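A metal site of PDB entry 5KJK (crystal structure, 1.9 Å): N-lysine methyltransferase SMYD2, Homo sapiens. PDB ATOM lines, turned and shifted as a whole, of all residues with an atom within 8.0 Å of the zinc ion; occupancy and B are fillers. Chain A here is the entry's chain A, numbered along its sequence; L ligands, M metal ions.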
ATOM      1  N   HIS A 203      32.543 -30.183 -24.490  1.00  0.00           N
ATOM      2  CA  HIS A 203      31.291 -29.510 -24.179  1.00  0.00           C
ATOM      3  C   HIS A 203      30.554 -28.936 -25.391  1.00  0.00           C
ATOM      4  O   HIS A 203      31.154 -28.409 -26.334  1.00  0.00           O
ATOM      5  CB  HIS A 203      31.552 -28.326 -23.221  1.00  0.00           C
ATOM      6  CG  HIS A 203      30.315 -27.501 -22.973  1.00  0.00           C
ATOM      7  ND1 HIS A 203      30.014 -26.398 -23.767  1.00  0.00           N
ATOM      8  CD2 HIS A 203      29.316 -27.698 -22.099  1.00  0.00           C
ATOM      9  CE1 HIS A 203      28.835 -25.970 -23.333  1.00  0.00           C
ATOM     10  NE2 HIS A 203      28.390 -26.708 -22.317  1.00  0.00           N
ATOM     11  N   SER A 204      29.213 -28.945 -25.292  1.00  0.00           N
ATOM     12  CA  SER A 204      28.305 -28.231 -26.186  1.00  0.00           C
ATOM     13  C   SER A 204      27.084 -27.829 -25.374  1.00  0.00           C
ATOM     14  O   SER A 204      26.683 -28.569 -24.485  1.00  0.00           O
ATOM     15  CB  SER A 204      27.867 -29.078 -27.373  1.00  0.00           C
ATOM     16  OG  SER A 204      26.909 -28.357 -28.144  1.00  0.00           O
ATOM     17  N   CYS A 205      26.495 -26.678 -25.695  1.00  0.00           N
ATOM     18  CA  CYS A 205      25.236 -26.179 -25.123  1.00  0.00           C
ATOM     19  C   CYS A 205      24.021 -26.852 -25.808  1.00  0.00           C
ATOM     20  O   CYS A 205      22.896 -26.696 -25.327  1.00  0.00           O
ATOM     21  CB  CYS A 205      25.162 -24.661 -25.214  1.00  0.00           C
ATOM     22  SG  CYS A 205      26.508 -23.828 -24.371  1.00  0.00           S
ATOM     23  N   CYS A 206      24.256 -27.605 -26.902  1.00  0.00           N
ATOM     24  CA  CYS A 206      23.238 -28.449 -27.556  1.00  0.00           C
ATOM     25  C   CYS A 206      23.860 -29.863 -27.625  1.00  0.00           C
ATOM     26  O   CYS A 206      24.277 -30.349 -28.676  1.00  0.00           O
ATOM     27  CB  CYS A 206      22.776 -27.910 -28.908  1.00  0.00           C
ATOM     28  SG  CYS A 206      24.088 -27.147 -29.877  1.00  0.00           S
ATOM     29  N   ILE A 237      27.655 -27.534 -18.042  1.00  0.00           N
ATOM     30  CA  ILE A 237      27.004 -26.548 -17.191  1.00  0.00           C
ATOM     31  C   ILE A 237      25.478 -26.584 -17.266  1.00  0.00           C
ATOM     32  O   ILE A 237      24.904 -27.241 -18.128  1.00  0.00           O
ATOM     33  CB  ILE A 237      27.538 -25.124 -17.624  1.00  0.00           C
ATOM     34  CG1 ILE A 237      27.452 -24.934 -19.160  1.00  0.00           C
ATOM     35  CG2 ILE A 237      28.962 -24.844 -17.110  1.00  0.00           C
ATOM     36  CD1 ILE A 237      27.321 -23.540 -19.615  1.00  0.00           C
ATOM     37  N   LEU A 239      22.236 -25.386 -18.498  1.00  0.00           N
ATOM     38  CA  LEU A 239      21.835 -24.776 -19.764  1.00  0.00           C
ATOM     39  C   LEU A 239      20.658 -23.802 -19.686  1.00  0.00           C
ATOM     40  O   LEU A 239      20.260 -23.247 -20.714  1.00  0.00           O
ATOM     41  CB  LEU A 239      21.561 -25.863 -20.811  1.00  0.00           C
ATOM     42  CG  LEU A 239      22.758 -26.762 -21.136  1.00  0.00           C
ATOM     43  CD1 LEU A 239      22.385 -27.855 -22.093  1.00  0.00           C
ATOM     44  CD2 LEU A 239      23.921 -25.938 -21.690  1.00  0.00           C
ATOM     45  N   THR A 243      23.545 -16.982 -23.251  1.00  0.00           N
ATOM     46  CA  THR A 243      24.878 -17.218 -23.814  1.00  0.00           C
ATOM     47  C   THR A 243      26.026 -16.563 -23.014  1.00  0.00           C
ATOM     48  O   THR A 243      27.023 -17.235 -22.729  1.00  0.00           O
ATOM     49  CB  THR A 243      24.888 -16.820 -25.285  1.00  0.00           C
ATOM     50  OG1 THR A 243      23.819 -17.520 -25.946  1.00  0.00           O
ATOM     51  CG2 THR A 243      26.222 -17.140 -25.965  1.00  0.00           C
ATOM     52  N   ARG A 246      26.526 -18.411 -19.639  1.00  0.00           N
ATOM     53  CA  ARG A 246      27.060 -19.751 -19.892  1.00  0.00           C
ATOM     54  C   ARG A 246      28.589 -19.707 -20.149  1.00  0.00           C
ATOM     55  O   ARG A 246      29.343 -20.464 -19.533  1.00  0.00           O
ATOM     56  CB  ARG A 246      26.337 -20.343 -21.109  1.00  0.00           C
ATOM     57  CG  ARG A 246      24.922 -20.822 -20.790  1.00  0.00           C
ATOM     58  CD  ARG A 246      24.421 -21.889 -21.753  1.00  0.00           C
ATOM     59  NE  ARG A 246      24.703 -21.592 -23.180  1.00  0.00           N
ATOM     60  CZ  ARG A 246      23.968 -20.793 -23.945  1.00  0.00           C
ATOM     61  NH1 ARG A 246      22.944 -20.114 -23.440  1.00  0.00           N
ATOM     62  NH2 ARG A 246      24.278 -20.627 -25.234  1.00  0.00           N
ATOM     63  N   ASN A 247      29.024 -18.762 -21.013  1.00  0.00           N
ATOM     64  CA  ASN A 247      30.414 -18.588 -21.411  1.00  0.00           C
ATOM     65  C   ASN A 247      31.240 -17.954 -20.293  1.00  0.00           C
ATOM     66  O   ASN A 247      32.412 -18.312 -20.180  1.00  0.00           O
ATOM     67  CB  ASN A 247      30.510 -17.842 -22.753  1.00  0.00           C
ATOM     68  CG  ASN A 247      30.333 -18.842 -23.851  1.00  0.00           C
ATOM     69  OD1 ASN A 247      31.047 -19.842 -23.908  1.00  0.00           O
ATOM     70  ND2 ASN A 247      29.284 -18.716 -24.642  1.00  0.00           N
ATOM     71  N   LEU A 250      31.868 -21.114 -18.345  1.00  0.00           N
ATOM     72  CA  LEU A 250      32.825 -21.980 -19.057  1.00  0.00           C
ATOM     73  C   LEU A 250      34.239 -21.395 -19.036  1.00  0.00           C
ATOM     74  O   LEU A 250      35.200 -22.146 -18.870  1.00  0.00           O
ATOM     75  CB  LEU A 250      32.357 -22.262 -20.495  1.00  0.00           C
ATOM     76  CG  LEU A 250      31.054 -23.068 -20.597  1.00  0.00           C
ATOM     77  CD1 LEU A 250      30.429 -22.927 -22.010  1.00  0.00           C
ATOM     78  CD2 LEU A 250      31.253 -24.504 -20.150  1.00  0.00           C
ATOM     79  N   PHE A 256      37.629 -21.843 -21.447  1.00  0.00           N
ATOM     80  CA  PHE A 256      37.328 -21.784 -22.882  1.00  0.00           C
ATOM     81  C   PHE A 256      36.006 -21.092 -23.105  1.00  0.00           C
ATOM     82  O   PHE A 256      35.215 -20.977 -22.171  1.00  0.00           O
ATOM     83  CB  PHE A 256      37.315 -23.215 -23.517  1.00  0.00           C
ATOM     84  CG  PHE A 256      36.043 -24.017 -23.280  1.00  0.00           C
ATOM     85  CD1 PHE A 256      34.988 -23.957 -24.195  1.00  0.00           C
ATOM     86  CD2 PHE A 256      35.915 -24.825 -22.160  1.00  0.00           C
ATOM     87  CE1 PHE A 256      33.794 -24.682 -23.967  1.00  0.00           C
ATOM     88  CE2 PHE A 256      34.735 -25.561 -21.946  1.00  0.00           C
ATOM     89  CZ  PHE A 256      33.689 -25.482 -22.853  1.00  0.00           C
ATOM     90  N   THR A 257      35.767 -20.662 -24.338  1.00  0.00           N
ATOM     91  CA  THR A 257      34.517 -20.065 -24.793  1.00  0.00           C
ATOM     92  C   THR A 257      33.924 -21.022 -25.810  1.00  0.00           C
ATOM     93  O   THR A 257      34.600 -21.443 -26.763  1.00  0.00           O
ATOM     94  CB  THR A 257      34.723 -18.666 -25.391  1.00  0.00           C
ATOM     95  OG1 THR A 257      35.228 -17.818 -24.369  1.00  0.00           O
ATOM     96  CG2 THR A 257      33.427 -18.052 -26.009  1.00  0.00           C
ATOM     97  N   CYS A 258      32.674 -21.368 -25.598  1.00  0.00           N
ATOM     98  CA  CYS A 258      31.922 -22.255 -26.459  1.00  0.00           C
ATOM     99  C   CYS A 258      31.492 -21.518 -27.697  1.00  0.00           C
ATOM    100  O   CYS A 258      31.074 -20.358 -27.625  1.00  0.00           O
ATOM    101  CB  CYS A 258      30.701 -22.818 -25.720  1.00  0.00           C
ATOM    102  SG  CYS A 258      29.820 -24.080 -26.671  1.00  0.00           S
ATOM    103  N   GLU A 259      31.557 -22.214 -28.832  1.00  0.00           N
ATOM    104  CA  GLU A 259      31.097 -21.712 -30.116  1.00  0.00           C
ATOM    105  C   GLU A 259      30.029 -22.666 -30.709  1.00  0.00           C
ATOM    106  O   GLU A 259      29.869 -22.709 -31.923  1.00  0.00           O
ATOM    107  CB  GLU A 259      32.264 -21.541 -31.125  1.00  0.00           C
ATOM    108  CG  GLU A 259      33.346 -20.568 -30.698  1.00  0.00           C
ATOM    109  CD  GLU A 259      34.494 -20.458 -31.683  1.00  0.00           C
ATOM    110  OE1 GLU A 259      35.590 -20.022 -31.260  1.00  0.00           O
ATOM    111  OE2 GLU A 259      34.320 -20.835 -32.863  1.00  0.00           O
ATOM    112  N   CYS A 260      29.301 -23.415 -29.870  1.00  0.00           N
ATOM    113  CA  CYS A 260      28.252 -24.305 -30.411  1.00  0.00           C
ATOM    114  C   CYS A 260      27.132 -23.490 -31.111  1.00  0.00           C
ATOM    115  O   CYS A 260      27.099 -22.252 -31.024  1.00  0.00           O
ATOM    116  CB  CYS A 260      27.672 -25.174 -29.311  1.00  0.00           C
ATOM    117  SG  CYS A 260      26.462 -24.308 -28.277  1.00  0.00           S
ATOM    118  N   GLN A 261      26.172 -24.185 -31.737  1.00  0.00           N
ATOM    119  CA  GLN A 261      25.069 -23.512 -32.442  1.00  0.00           C
ATOM    120  C   GLN A 261      24.261 -22.576 -31.528  1.00  0.00           C
ATOM    121  O   GLN A 261      23.940 -21.478 -31.954  1.00  0.00           O
ATOM    122  CB  GLN A 261      24.171 -24.494 -33.201  1.00  0.00           C
ATOM    123  CG  GLN A 261      23.582 -23.889 -34.483  1.00  0.00           C
ATOM    124  CD  GLN A 261      24.648 -23.444 -35.478  1.00  0.00           C
ATOM    125  OE1 GLN A 261      25.469 -24.241 -35.958  1.00  0.00           O
ATOM    126  NE2 GLN A 261      24.708 -22.145 -35.764  1.00  0.00           N
ATOM    127  N   GLU A 262      24.048 -22.963 -30.270  1.00  0.00           N
ATOM    128  CA  GLU A 262      23.319 -22.139 -29.285  1.00  0.00           C
ATOM    129  C   GLU A 262      24.067 -20.824 -28.953  1.00  0.00           C
ATOM    130  O   GLU A 262      23.448 -19.772 -28.870  1.00  0.00           O
ATOM    131  CB  GLU A 262      23.026 -22.934 -28.003  1.00  0.00           C
ATOM    132  CG  GLU A 262      22.067 -24.098 -28.198  1.00  0.00           C
ATOM    133  CD  GLU A 262      20.594 -23.802 -28.501  1.00  0.00           C
ATOM    134  OE1 GLU A 262      20.177 -22.618 -28.447  1.00  0.00           O
ATOM    135  OE2 GLU A 262      19.845 -24.766 -28.766  1.00  0.00           O
ATOM    136  N   CYS A 263      25.390 -20.928 -28.760  1.00  0.00           N
ATOM    137  CA  CYS A 263      26.273 -19.801 -28.457  1.00  0.00           C
ATOM    138  C   CYS A 263      26.486 -18.874 -29.686  1.00  0.00           C
ATOM    139  O   CYS A 263      26.574 -17.654 -29.542  1.00  0.00           O
ATOM    140  CB  CYS A 263      27.596 -20.309 -27.864  1.00  0.00           C
ATOM    141  SG  CYS A 263      27.411 -21.125 -26.243  1.00  0.00           S
ATOM    142  N   THR A 264      26.472 -19.458 -30.892  1.00  0.00           N
ATOM    143  CA  THR A 264      26.672 -18.702 -32.137  1.00  0.00           C
ATOM    144  C   THR A 264      25.388 -17.945 -32.532  1.00  0.00           C
ATOM    145  O   THR A 264      25.418 -16.736 -32.789  1.00  0.00           O
ATOM    146  CB  THR A 264      27.223 -19.632 -33.247  1.00  0.00           C
ATOM    147  OG1 THR A 264      28.460 -20.194 -32.797  1.00  0.00           O
ATOM    148  CG2 THR A 264      27.474 -18.908 -34.576  1.00  0.00           C
HETATM  149  N1  LIG L   1      39.502 -31.655 -24.814  1.00  0.00           N
HETATM  150  C1  LIG L   1      39.906 -32.213 -23.508  1.00  0.00           C
HETATM  151  C2  LIG L   1      41.344 -32.881 -23.530  1.00  0.00           C
HETATM  152  O1  LIG L   1      42.003 -32.780 -24.595  1.00  0.00           O
HETATM  153  O2  LIG L   1      41.737 -33.430 -22.483  1.00  0.00           O
HETATM  154  C3  LIG L   1      38.830 -33.184 -22.968  1.00  0.00           C
HETATM  155  C4  LIG L   1      37.737 -32.463 -22.191  1.00  0.00           C
HETATM  156  S1  LIG L   1      38.418 -31.809 -20.644  1.00  0.00           S
HETATM  157  C5  LIG L   1      37.338 -32.399 -19.433  1.00  0.00           C
HETATM  158  C6  LIG L   1      37.802 -30.133 -20.644  1.00  0.00           C
HETATM  159  C7  LIG L   1      38.623 -29.176 -21.484  1.00  0.00           C
HETATM  160  O3  LIG L   1      38.392 -29.416 -22.890  1.00  0.00           O
HETATM  161  C8  LIG L   1      38.262 -27.709 -21.290  1.00  0.00           C
HETATM  162  O4  LIG L   1      38.800 -27.174 -20.094  1.00  0.00           O
HETATM  163  C9  LIG L   1      38.720 -27.086 -22.607  1.00  0.00           C
HETATM  164  O5  LIG L   1      40.116 -26.838 -22.697  1.00  0.00           O
HETATM  165  C10 LIG L   1      38.340 -28.187 -23.608  1.00  0.00           C
HETATM  166  N2  LIG L   1      37.010 -28.046 -24.200  1.00  0.00           N
HETATM  167  C11 LIG L   1      35.880 -28.767 -23.909  1.00  0.00           C
HETATM  168  N3  LIG L   1      34.844 -28.444 -24.647  1.00  0.00           N
HETATM  169  C12 LIG L   1      35.308 -27.431 -25.468  1.00  0.00           C
HETATM  170  C13 LIG L   1      34.695 -26.652 -26.472  1.00  0.00           C
HETATM  171  N4  LIG L   1      33.429 -26.835 -26.887  1.00  0.00           N
HETATM  172  N5  LIG L   1      35.435 -25.695 -27.075  1.00  0.00           N
HETATM  173  C14 LIG L   1      36.717 -25.540 -26.701  1.00  0.00           C
HETATM  174  N6  LIG L   1      37.408 -26.231 -25.787  1.00  0.00           N
HETATM  175  C15 LIG L   1      36.649 -27.174 -25.205  1.00  0.00           C
HETATM  176 ZN    ZN M   1      27.631 -23.263 -26.472  1.00  0.00          ZN
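The backbone NH (N) of His 203 is in hydrogen-bond range of a nitrogen (N3) of the ligand, 2.9 Å away.
O of His 203 lies within hydrogen-bond range of N4 of the ligand (2.8 Å).
The side-chain sulfur (SG) of Cys 263 sits close to the guanidinium group (NH2) of Arg 246 (3.3 Å).
The side-chain amide nitrogen of Asn 247 lies close to the side-chain sulfur of Cys 263.
A ring nitrogen (ND1) of His 203 lies close to the side-chain sulfur (SG) of Cys 258.
The backbone NH (N) of Cys 258 sits at hydrogen-bond distance from the side-chain amide oxygen (OD1) of Asn 247 (2.8 Å).
SG of Cys 260 lies close to N of Glu 262.
The backbone carbonyl oxygen (O) of Cys 260 sits at hydrogen-bond distance from the side-chain hydroxyl (OG1) of Thr 264, at 3.0 Å.
The side-chain sulfur (SG) of Cys 205 lies close to the guanidinium group (NE) of Arg 246.
The nearest printed residue that does not touch the zinc ion is His 203 (4.3 Å).
The zinc ion is bound by the side-chain sulfur (SG) of Cys 263 (2.2 Å), the side-chain sulfur (SG) of Cys 258 (2.3 Å), the side-chain sulfur (SG) of Cys 260 (2.4 Å) and the side-chain sulfur (SG) of Cys 205 (2.4 Å).
The zinc ion has four donor atoms within binding distance.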
